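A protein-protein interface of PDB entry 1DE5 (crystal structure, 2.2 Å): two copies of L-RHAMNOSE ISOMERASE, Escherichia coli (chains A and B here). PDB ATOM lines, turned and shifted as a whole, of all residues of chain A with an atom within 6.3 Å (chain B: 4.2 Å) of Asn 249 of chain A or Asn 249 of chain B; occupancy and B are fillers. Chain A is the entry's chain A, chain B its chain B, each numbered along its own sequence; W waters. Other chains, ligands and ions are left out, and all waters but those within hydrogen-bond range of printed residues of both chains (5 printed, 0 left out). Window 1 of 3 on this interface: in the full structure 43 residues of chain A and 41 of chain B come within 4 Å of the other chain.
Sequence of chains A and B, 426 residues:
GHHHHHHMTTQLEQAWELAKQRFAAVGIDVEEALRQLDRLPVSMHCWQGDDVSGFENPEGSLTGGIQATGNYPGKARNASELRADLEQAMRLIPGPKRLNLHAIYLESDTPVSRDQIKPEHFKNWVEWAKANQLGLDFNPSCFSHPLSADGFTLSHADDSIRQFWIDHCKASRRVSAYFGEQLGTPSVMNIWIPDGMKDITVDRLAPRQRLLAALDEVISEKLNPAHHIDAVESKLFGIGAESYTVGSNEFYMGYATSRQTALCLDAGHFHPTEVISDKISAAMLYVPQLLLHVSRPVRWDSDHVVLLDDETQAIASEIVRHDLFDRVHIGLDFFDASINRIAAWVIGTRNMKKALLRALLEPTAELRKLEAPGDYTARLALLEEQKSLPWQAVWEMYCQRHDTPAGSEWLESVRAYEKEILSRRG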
ATOM      1  N   SER A 234      13.769  -3.605 -29.003  1.00  0.00           N
ATOM      2  CA  SER A 234      13.033  -3.692 -30.273  1.00  0.00           C
ATOM      3  C   SER A 234      13.251  -2.431 -31.121  1.00  0.00           C
ATOM      4  O   SER A 234      13.617  -1.394 -30.589  1.00  0.00           O
ATOM      5  CB  SER A 234      11.531  -3.873 -30.092  1.00  0.00           C
ATOM      6  OG  SER A 234      10.906  -2.604 -29.883  1.00  0.00           O
ATOM      7  N   LYS A 235      13.036  -2.561 -32.440  1.00  0.00           N
ATOM      8  CA  LYS A 235      13.182  -1.475 -33.405  1.00  0.00           C
ATOM      9  C   LYS A 235      12.156  -1.710 -34.462  1.00  0.00           C
ATOM     10  O   LYS A 235      11.802  -2.881 -34.703  1.00  0.00           O
ATOM     11  CB  LYS A 235      14.548  -1.419 -34.056  1.00  0.00           C
ATOM     12  CG  LYS A 235      14.920  -0.021 -34.505  1.00  0.00           C
ATOM     13  CD  LYS A 235      16.299   0.018 -35.167  1.00  0.00           C
ATOM     14  CE  LYS A 235      16.646   1.373 -35.739  1.00  0.00           C
ATOM     15  NZ  LYS A 235      18.090   1.648 -35.939  1.00  0.00           N
ATOM     16  N   LEU A 236      11.704  -0.593 -35.025  1.00  0.00           N
ATOM     17  CA  LEU A 236      10.677  -0.610 -36.051  1.00  0.00           C
ATOM     18  C   LEU A 236      11.286  -0.712 -37.466  1.00  0.00           C
ATOM     19  O   LEU A 236      10.967  -1.583 -38.298  1.00  0.00           O
ATOM     20  CB  LEU A 236       9.791   0.668 -35.879  1.00  0.00           C
ATOM     21  CG  LEU A 236       8.764   0.896 -37.010  1.00  0.00           C
ATOM     22  CD1 LEU A 236       7.782  -0.283 -37.087  1.00  0.00           C
ATOM     23  CD2 LEU A 236       8.048   2.257 -36.890  1.00  0.00           C
ATOM     24  N   GLY A 247      13.549  -8.275 -34.757  1.00  0.00           N
ATOM     25  CA  GLY A 247      13.209  -8.077 -33.364  1.00  0.00           C
ATOM     26  C   GLY A 247      12.292  -6.922 -33.253  1.00  0.00           C
ATOM     27  O   GLY A 247      12.702  -5.825 -32.960  1.00  0.00           O
ATOM     28  N   SER A 248      11.053  -7.189 -33.557  1.00  0.00           N
ATOM     29  CA  SER A 248      10.025  -6.146 -33.500  1.00  0.00           C
ATOM     30  C   SER A 248       9.531  -5.921 -32.055  1.00  0.00           C
ATOM     31  O   SER A 248       9.907  -6.629 -31.090  1.00  0.00           O
ATOM     32  CB  SER A 248       8.867  -6.651 -34.301  1.00  0.00           C
ATOM     33  OG  SER A 248       8.526  -7.919 -33.779  1.00  0.00           O
ATOM     34  N   ASN A 249       8.655  -4.948 -31.869  1.00  0.00           N
ATOM     35  CA  ASN A 249       8.167  -4.709 -30.529  1.00  0.00           C
ATOM     36  C   ASN A 249       7.549  -5.976 -29.940  1.00  0.00           C
ATOM     37  O   ASN A 249       8.026  -6.527 -28.941  1.00  0.00           O
ATOM     38  CB  ASN A 249       7.216  -3.507 -30.559  1.00  0.00           C
ATOM     39  CG  ASN A 249       6.219  -3.381 -29.427  1.00  0.00           C
ATOM     40  OD1 ASN A 249       6.213  -4.073 -28.398  1.00  0.00           O
ATOM     41  ND2 ASN A 249       5.444  -2.343 -29.552  1.00  0.00           N
ATOM     42  N   GLU A 250       6.475  -6.451 -30.540  1.00  0.00           N
ATOM     43  CA  GLU A 250       5.870  -7.650 -30.041  1.00  0.00           C
ATOM     44  C   GLU A 250       6.874  -8.778 -29.853  1.00  0.00           C
ATOM     45  O   GLU A 250       6.740  -9.577 -28.938  1.00  0.00           O
ATOM     46  CB  GLU A 250       4.827  -8.144 -31.051  1.00  0.00           C
ATOM     47  CG  GLU A 250       3.660  -7.156 -31.101  1.00  0.00           C
ATOM     48  CD  GLU A 250       3.918  -5.865 -31.808  1.00  0.00           C
ATOM     49  OE1 GLU A 250       3.175  -4.919 -31.647  1.00  0.00           O
ATOM     50  OE2 GLU A 250       4.907  -5.888 -32.679  1.00  0.00           O
ATOM     51  N   PHE A 251       7.878  -8.852 -30.732  1.00  0.00           N
ATOM     52  CA  PHE A 251       8.893  -9.909 -30.652  1.00  0.00           C
ATOM     53  C   PHE A 251       9.590 -10.058 -29.273  1.00  0.00           C
ATOM     54  O   PHE A 251       9.690 -11.157 -28.663  1.00  0.00           O
ATOM     55  CB  PHE A 251       9.896  -9.949 -31.847  1.00  0.00           C
ATOM     56  CG  PHE A 251      10.860 -11.108 -31.654  1.00  0.00           C
ATOM     57  CD1 PHE A 251      10.596 -12.383 -32.165  1.00  0.00           C
ATOM     58  CD2 PHE A 251      11.998 -10.940 -30.866  1.00  0.00           C
ATOM     59  CE1 PHE A 251      11.461 -13.456 -31.912  1.00  0.00           C
ATOM     60  CE2 PHE A 251      12.891 -11.992 -30.647  1.00  0.00           C
ATOM     61  CZ  PHE A 251      12.628 -13.263 -31.165  1.00  0.00           C
ATOM     62  N   TYR A 252      10.030  -8.895 -28.801  1.00  0.00           N
ATOM     63  CA  TYR A 252      10.740  -8.729 -27.546  1.00  0.00           C
ATOM     64  C   TYR A 252       9.815  -8.605 -26.372  1.00  0.00           C
ATOM     65  O   TYR A 252      10.144  -9.053 -25.271  1.00  0.00           O
ATOM     66  CB  TYR A 252      11.708  -7.570 -27.590  1.00  0.00           C
ATOM     67  CG  TYR A 252      12.893  -7.816 -28.490  1.00  0.00           C
ATOM     68  CD1 TYR A 252      13.258  -6.839 -29.416  1.00  0.00           C
ATOM     69  CD2 TYR A 252      13.653  -8.985 -28.385  1.00  0.00           C
ATOM     70  CE1 TYR A 252      14.357  -7.008 -30.257  1.00  0.00           C
ATOM     71  CE2 TYR A 252      14.774  -9.158 -29.195  1.00  0.00           C
ATOM     72  CZ  TYR A 252      15.116  -8.170 -30.123  1.00  0.00           C
ATOM     73  OH  TYR A 252      16.170  -8.365 -30.934  1.00  0.00           O
ATOM     74  N   MET A 253       8.647  -8.029 -26.603  1.00  0.00           N
ATOM     75  CA  MET A 253       7.771  -7.996 -25.463  1.00  0.00           C
ATOM     76  C   MET A 253       7.512  -9.479 -25.159  1.00  0.00           C
ATOM     77  O   MET A 253       7.690  -9.997 -24.049  1.00  0.00           O
ATOM     78  CB  MET A 253       6.423  -7.266 -25.712  1.00  0.00           C
ATOM     79  CG  MET A 253       5.495  -7.406 -24.479  1.00  0.00           C
ATOM     80  SD  MET A 253       6.051  -6.254 -23.213  1.00  0.00           S
ATOM     81  CE  MET A 253       5.066  -6.758 -21.781  1.00  0.00           C
ATOM     82  N   GLY A 254       7.135 -10.218 -26.186  1.00  0.00           N
ATOM     83  CA  GLY A 254       6.899 -11.634 -25.976  1.00  0.00           C
ATOM     84  C   GLY A 254       8.151 -12.296 -25.360  1.00  0.00           C
ATOM     85  O   GLY A 254       8.077 -13.087 -24.422  1.00  0.00           O
ATOM     86  N   LEU A 263      13.351  -5.506 -20.540  1.00  0.00           N
ATOM     87  CA  LEU A 263      12.896  -5.064 -21.822  1.00  0.00           C
ATOM     88  C   LEU A 263      13.412  -3.668 -22.059  1.00  0.00           C
ATOM     89  O   LEU A 263      13.293  -2.815 -21.182  1.00  0.00           O
ATOM     90  CB  LEU A 263      11.360  -5.119 -21.927  1.00  0.00           C
ATOM     91  CG  LEU A 263      10.886  -4.454 -23.221  1.00  0.00           C
ATOM     92  CD1 LEU A 263      11.220  -5.387 -24.381  1.00  0.00           C
ATOM     93  CD2 LEU A 263       9.373  -4.302 -23.176  1.00  0.00           C
ATOM     94  N   LEU A 265      13.280  -0.133 -24.012  1.00  0.00           N
ATOM     95  CA  LEU A 265      12.337   0.747 -24.703  1.00  0.00           C
ATOM     96  C   LEU A 265      13.093   1.971 -25.198  1.00  0.00           C
ATOM     97  O   LEU A 265      13.519   2.793 -24.396  1.00  0.00           O
ATOM     98  CB  LEU A 265      11.150   1.169 -23.747  1.00  0.00           C
ATOM     99  CG  LEU A 265      10.185   0.024 -23.328  1.00  0.00           C
ATOM    100  CD1 LEU A 265       9.170   0.451 -22.273  1.00  0.00           C
ATOM    101  CD2 LEU A 265       9.413  -0.486 -24.533  1.00  0.00           C
ATOM    102  N   PHE A 270       9.852   3.595 -32.479  1.00  0.00           N
ATOM    103  CA  PHE A 270       8.498   3.181 -32.691  1.00  0.00           C
ATOM    104  C   PHE A 270       7.793   3.968 -33.750  1.00  0.00           C
ATOM    105  O   PHE A 270       8.434   4.755 -34.450  1.00  0.00           O
ATOM    106  CB  PHE A 270       7.753   3.213 -31.337  1.00  0.00           C
ATOM    107  CG  PHE A 270       8.312   2.239 -30.318  1.00  0.00           C
ATOM    108  CD1 PHE A 270       7.709   0.993 -30.140  1.00  0.00           C
ATOM    109  CD2 PHE A 270       9.457   2.530 -29.567  1.00  0.00           C
ATOM    110  CE1 PHE A 270       8.188   0.079 -29.194  1.00  0.00           C
ATOM    111  CE2 PHE A 270       9.965   1.633 -28.620  1.00  0.00           C
ATOM    112  CZ  PHE A 270       9.315   0.413 -28.435  1.00  0.00           C
ATOM    113  N   GLU A 274       3.879   7.008 -31.665  1.00  0.00           N
ATOM    114  CA  GLU A 274       3.945   6.033 -30.570  1.00  0.00           C
ATOM    115  C   GLU A 274       4.889   6.561 -29.476  1.00  0.00           C
ATOM    116  O   GLU A 274       5.923   7.122 -29.791  1.00  0.00           O
ATOM    117  CB  GLU A 274       4.389   4.683 -31.105  1.00  0.00           C
ATOM    118  CG  GLU A 274       4.323   3.514 -30.106  1.00  0.00           C
ATOM    119  CD  GLU A 274       4.397   2.236 -30.866  1.00  0.00           C
ATOM    120  OE1 GLU A 274       4.006   1.168 -30.451  1.00  0.00           O
ATOM    121  OE2 GLU A 274       4.910   2.430 -32.057  1.00  0.00           O
ATOM    122  N   ASP A 278       4.128   5.643 -22.302  1.00  0.00           N
ATOM    123  CA  ASP A 278       2.913   4.847 -22.144  1.00  0.00           C
ATOM    124  C   ASP A 278       3.194   3.417 -21.795  1.00  0.00           C
ATOM    125  O   ASP A 278       2.371   2.766 -21.138  1.00  0.00           O
ATOM    126  CB  ASP A 278       2.074   4.826 -23.477  1.00  0.00           C
ATOM    127  CG  ASP A 278       0.845   3.962 -23.357  1.00  0.00           C
ATOM    128  OD1 ASP A 278      -0.053   4.234 -22.575  1.00  0.00           O
ATOM    129  OD2 ASP A 278       0.932   2.816 -24.039  1.00  0.00           O
ATOM    130  N   LYS A 279       4.314   2.909 -22.349  1.00  0.00           N
ATOM    131  CA  LYS A 279       4.680   1.493 -22.241  1.00  0.00           C
ATOM    132  C   LYS A 279       5.168   1.015 -20.922  1.00  0.00           C
ATOM    133  O   LYS A 279       4.873  -0.136 -20.576  1.00  0.00           O
ATOM    134  CB  LYS A 279       5.512   1.008 -23.388  1.00  0.00           C
ATOM    135  CG  LYS A 279       5.014   1.613 -24.705  1.00  0.00           C
ATOM    136  CD  LYS A 279       5.918   1.359 -25.889  1.00  0.00           C
ATOM    137  CE  LYS A 279       5.327   1.787 -27.230  1.00  0.00           C
ATOM    138  NZ  LYS A 279       4.160   1.003 -27.620  1.00  0.00           N
ATOM    139  N   SER B 234      -6.035  -5.641 -27.657  1.00  0.00           N
ATOM    140  CA  SER B 234      -5.663  -4.289 -27.256  1.00  0.00           C
ATOM    141  C   SER B 234      -6.205  -3.291 -28.253  1.00  0.00           C
ATOM    142  O   SER B 234      -6.641  -3.661 -29.343  1.00  0.00           O
ATOM    143  CB  SER B 234      -4.174  -4.020 -27.235  1.00  0.00           C
ATOM    144  OG  SER B 234      -3.758  -4.335 -28.535  1.00  0.00           O
ATOM    145  N   SER B 248      -3.393  -1.969 -23.313  1.00  0.00           N
ATOM    146  CA  SER B 248      -2.656  -1.556 -24.488  1.00  0.00           C
ATOM    147  C   SER B 248      -2.079  -2.770 -25.214  1.00  0.00           C
ATOM    148  O   SER B 248      -2.256  -3.911 -24.790  1.00  0.00           O
ATOM    149  CB  SER B 248      -1.528  -0.648 -24.025  1.00  0.00           C
ATOM    150  OG  SER B 248      -0.694  -1.413 -23.171  1.00  0.00           O
ATOM    151  N   ASN B 249      -1.358  -2.496 -26.294  1.00  0.00           N
ATOM    152  CA  ASN B 249      -0.671  -3.515 -27.033  1.00  0.00           C
ATOM    153  C   ASN B 249       0.305  -4.272 -26.096  1.00  0.00           C
ATOM    154  O   ASN B 249       0.253  -5.512 -25.932  1.00  0.00           O
ATOM    155  CB  ASN B 249       0.140  -2.806 -28.135  1.00  0.00           C
ATOM    156  CG  ASN B 249       1.073  -3.716 -28.917  1.00  0.00           C
ATOM    157  OD1 ASN B 249       1.265  -4.923 -28.620  1.00  0.00           O
ATOM    158  ND2 ASN B 249       1.676  -3.123 -29.949  1.00  0.00           N
ATOM    159  N   GLU B 250       1.246  -3.539 -25.470  1.00  0.00           N
ATOM    160  CA  GLU B 250       2.186  -4.225 -24.564  1.00  0.00           C
ATOM    161  C   GLU B 250       1.471  -4.970 -23.430  1.00  0.00           C
ATOM    162  O   GLU B 250       1.795  -6.125 -23.154  1.00  0.00           O
ATOM    163  CB  GLU B 250       3.238  -3.298 -24.022  1.00  0.00           C
ATOM    164  CG  GLU B 250       4.197  -2.823 -25.139  1.00  0.00           C
ATOM    165  CD  GLU B 250       3.602  -1.804 -26.062  1.00  0.00           C
ATOM    166  OE1 GLU B 250       4.200  -1.399 -27.007  1.00  0.00           O
ATOM    167  OE2 GLU B 250       2.443  -1.325 -25.690  1.00  0.00           O
ATOM    168  N   PHE B 251       0.477  -4.348 -22.804  1.00  0.00           N
ATOM    169  CA  PHE B 251      -0.334  -5.000 -21.737  1.00  0.00           C
ATOM    170  C   PHE B 251      -0.812  -6.419 -22.144  1.00  0.00           C
ATOM    171  O   PHE B 251      -0.615  -7.448 -21.503  1.00  0.00           O
ATOM    172  CB  PHE B 251      -1.582  -4.074 -21.364  1.00  0.00           C
ATOM    173  CG  PHE B 251      -2.328  -4.698 -20.210  1.00  0.00           C
ATOM    174  CD1 PHE B 251      -1.976  -4.438 -18.883  1.00  0.00           C
ATOM    175  CD2 PHE B 251      -3.249  -5.711 -20.459  1.00  0.00           C
ATOM    176  CE1 PHE B 251      -2.598  -5.114 -17.840  1.00  0.00           C
ATOM    177  CE2 PHE B 251      -3.877  -6.411 -19.432  1.00  0.00           C
ATOM    178  CZ  PHE B 251      -3.559  -6.089 -18.117  1.00  0.00           C
ATOM    179  N   TYR B 252      -1.476  -6.518 -23.290  1.00  0.00           N
ATOM    180  CA  TYR B 252      -2.028  -7.785 -23.763  1.00  0.00           C
ATOM    181  C   TYR B 252      -1.048  -8.738 -24.425  1.00  0.00           C
ATOM    182  O   TYR B 252      -1.244  -9.963 -24.523  1.00  0.00           O
ATOM    183  CB  TYR B 252      -3.148  -7.461 -24.768  1.00  0.00           C
ATOM    184  CG  TYR B 252      -4.436  -7.077 -24.091  1.00  0.00           C
ATOM    185  CD1 TYR B 252      -5.156  -5.986 -24.579  1.00  0.00           C
ATOM    186  CD2 TYR B 252      -4.907  -7.769 -22.967  1.00  0.00           C
ATOM    187  CE1 TYR B 252      -6.368  -5.627 -23.991  1.00  0.00           C
ATOM    188  CE2 TYR B 252      -6.123  -7.429 -22.371  1.00  0.00           C
ATOM    189  CZ  TYR B 252      -6.853  -6.355 -22.897  1.00  0.00           C
ATOM    190  OH  TYR B 252      -8.055  -5.977 -22.334  1.00  0.00           O
ATOM    191  N   MET B 253      -0.009  -8.185 -24.975  1.00  0.00           N
ATOM    192  CA  MET B 253       0.944  -9.117 -25.525  1.00  0.00           C
ATOM    193  C   MET B 253       1.473  -9.776 -24.222  1.00  0.00           C
ATOM    194  O   MET B 253       1.509 -11.014 -24.075  1.00  0.00           O
ATOM    195  CB  MET B 253       2.054  -8.332 -26.283  1.00  0.00           C
ATOM    196  CG  MET B 253       3.219  -9.213 -26.735  1.00  0.00           C
ATOM    197  SD  MET B 253       2.638 -10.366 -27.988  1.00  0.00           S
ATOM    198  CE  MET B 253       3.753 -11.787 -27.788  1.00  0.00           C
ATOM    199  N   PHE B 270      -4.135   0.126 -34.084  1.00  0.00           N
ATOM    200  CA  PHE B 270      -2.776   0.582 -33.841  1.00  0.00           C
ATOM    201  C   PHE B 270      -2.420   2.005 -34.223  1.00  0.00           C
ATOM    202  O   PHE B 270      -3.276   2.832 -34.502  1.00  0.00           O
ATOM    203  CB  PHE B 270      -1.805  -0.419 -34.458  1.00  0.00           C
ATOM    204  CG  PHE B 270      -1.971  -1.698 -33.708  1.00  0.00           C
ATOM    205  CD1 PHE B 270      -1.166  -2.005 -32.605  1.00  0.00           C
ATOM    206  CD2 PHE B 270      -2.998  -2.572 -34.072  1.00  0.00           C
ATOM    207  CE1 PHE B 270      -1.355  -3.200 -31.893  1.00  0.00           C
ATOM    208  CE2 PHE B 270      -3.166  -3.788 -33.390  1.00  0.00           C
ATOM    209  CZ  PHE B 270      -2.378  -4.081 -32.271  1.00  0.00           C
ATOM    210  N   GLU B 274       1.150   1.594 -38.411  1.00  0.00           N
ATOM    211  CA  GLU B 274       1.432   0.316 -37.818  1.00  0.00           C
ATOM    212  C   GLU B 274       0.610  -0.797 -38.461  1.00  0.00           C
ATOM    213  O   GLU B 274      -0.534  -0.566 -38.802  1.00  0.00           O
ATOM    214  CB  GLU B 274       1.295   0.389 -36.308  1.00  0.00           C
ATOM    215  CG  GLU B 274       1.424  -0.983 -35.627  1.00  0.00           C
ATOM    216  CD  GLU B 274       1.604  -0.743 -34.148  1.00  0.00           C
ATOM    217  OE1 GLU B 274       2.086  -1.531 -33.338  1.00  0.00           O
ATOM    218  OE2 GLU B 274       1.201   0.461 -33.846  1.00  0.00           O
ATOM    219  N   LYS B 279       2.978  -8.334 -37.231  1.00  0.00           N
ATOM    220  CA  LYS B 279       2.765  -8.899 -35.903  1.00  0.00           C
ATOM    221  C   LYS B 279       2.448 -10.378 -35.903  1.00  0.00           C
ATOM    222  O   LYS B 279       2.744 -11.134 -34.965  1.00  0.00           O
ATOM    223  CB  LYS B 279       1.688  -8.081 -35.200  1.00  0.00           C
ATOM    224  CG  LYS B 279       2.153  -6.652 -35.041  1.00  0.00           C
ATOM    225  CD  LYS B 279       1.087  -5.777 -34.462  1.00  0.00           C
ATOM    226  CE  LYS B 279       1.439  -4.324 -34.621  1.00  0.00           C
ATOM    227  NZ  LYS B 279       2.626  -3.891 -33.873  1.00  0.00           N
HETATM  228  O   HOH W   1       1.446   0.036 -23.510  1.00  0.00           O
HETATM  229  O   HOH W   2       3.980  -5.659 -27.736  1.00  0.00           O
HETATM  230  O   HOH W   3       4.835  -0.689 -31.797  1.00  0.00           O
HETATM  231  O   HOH W   4       1.560  -0.344 -30.706  1.00  0.00           O
HETATM  232  O   HOH W   5       5.347  -3.150 -33.738  1.00  0.00           O
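Asn 249 of chain A touches its own counterpart, Asn 249 of chain B. Asn 249 of chain A touches Glu 250 of chain B, and with the chains exchanged Glu 250 of chain A touches Asn 249 of chain B. Glu 250 of chain A touches Glu 274 of chain B, but with the chains exchanged Glu 274 of chain A does not touch Glu 250 of chain B (4.3 Å). Met 253 of chain B touches its own counterpart, Met 253 of chain A. Positions printed for both chains: 234, 248, 249, 250, 251, 252, 253, 270, 274 and 279.
Lys 235 of chain A touches none of the printed residues of chain B. Asn 249 of chain A touches just these residues of chain B: Asn 249 (3.9 Å) and Glu 250 (3.0 Å). Asn 249 of chain B touches just these residues of chain A: Asn 249 and Glu 250. Of the printed residues of chain A, Glu 250 of chain B touches Asn 249 (3.0 Å), Met 253 (3.6 Å) and Lys 279 (2.5 Å). Of the printed residues of chain A, Met 253 of chain B touches Glu 250 (3.9 Å), Met 253 (3.7 Å) and Gly 254 (3.6 Å). Of the printed residues of chain A, Glu 274 of chain B touches Glu 250 (3.9 Å). The nearest residue of chain A that does not touch Asn 249 of chain B is Glu 274 of chain A (4.9 Å).
ND2 of Asn 249 of chain A touches ND2 of Asn 249 of chain B (3.9 Å). O of Glu 250 of chain A touches CE of Met 253 of chain B, at 3.9 Å. Glu 250 of chain A touches Glu 274 of chain B (OE1 to OE1, 3.9 Å). Met 253 of chain A touches Glu 250 of chain B. Met 253 of chain A touches Met 253 of chain B (CG to CG, 3.7 Å). CA of Gly 254 of chain A touches CE of Met 253 of chain B, 3.6 Å away.
Water W3 lies within hydrogen-bond range of the side-chain carboxylate (OE1) of Glu 274 of chain A, the side-chain amide nitrogen (ND2) of Asn 249 of chain A and the side-chain carboxylate (OE1) of Glu 274 of chain B. Water W1 lies within hydrogen-bond range of the side-chain hydroxyl (OG) of Ser 248 of chain B, the side-chain carboxylate (OE2) of Glu 250 of chain B and the side-chain carboxylate (OD2) of Asp 278 of chain A. Water W2 lies within hydrogen-bond range of OD1 of Asn 249 of chain A (2.8 Å) and OD1 of Asn 249 of chain B (2.9 Å). Water W5 lies within hydrogen-bond range of the side-chain amino group of Lys 279 of chain B (2.8 Å) and the side-chain carboxylate of Glu 250 of chain A (3.0 Å). Water W4 lies within hydrogen-bond range of ND2 of Asn 249 of chain B (2.9 Å), OE1 of Glu 274 of chain A (2.9 Å) and OE1 of Glu 274 of chain B (2.9 Å).
Hydrophobic or aromatic side chains of chain A that line the printed part of chain B: Met 253. Hydrophobic or aromatic side chains of chain B that line the printed part of chain A: Met 253. Among the printed residues, Asp or Glu carboxylates within 4 Å of a Lys or Arg side-chain nitrogen of the other chain: Glu 250 of chain A with Lys 279 of chain B (2.5 Å) and Lys 279 of chain A with Glu 250 of chain B (2.5 Å).
OE1 of Glu 274 of chain B is in salt-bridge range of NZ of Lys 279 of chain B, at 2.5 Å. The side-chain amino group (NZ) of Lys 279 of chain A is in salt-bridge range of the side-chain carboxylate (OE1) of Glu 274 of chain A (2.8 Å).
The side-chain carboxylate (OE1) of Glu 250 of chain A lies within hydrogen-bond range of the side-chain amide nitrogen (ND2) of Asn 249 of chain B, at 2.9 Å. OE1 of Glu 250 of chain B lies within hydrogen-bond range of ND2 of Asn 249 of chain A. The side-chain amino group of Lys 279 of chain A is in salt-bridge range of the side-chain carboxylate of Glu 250 of chain B, at 2.5 Å. The side-chain carboxylate (OE1) of Glu 250 of chain A is in salt-bridge range of the side-chain amino group (NZ) of Lys 279 of chain B (2.5 Å).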
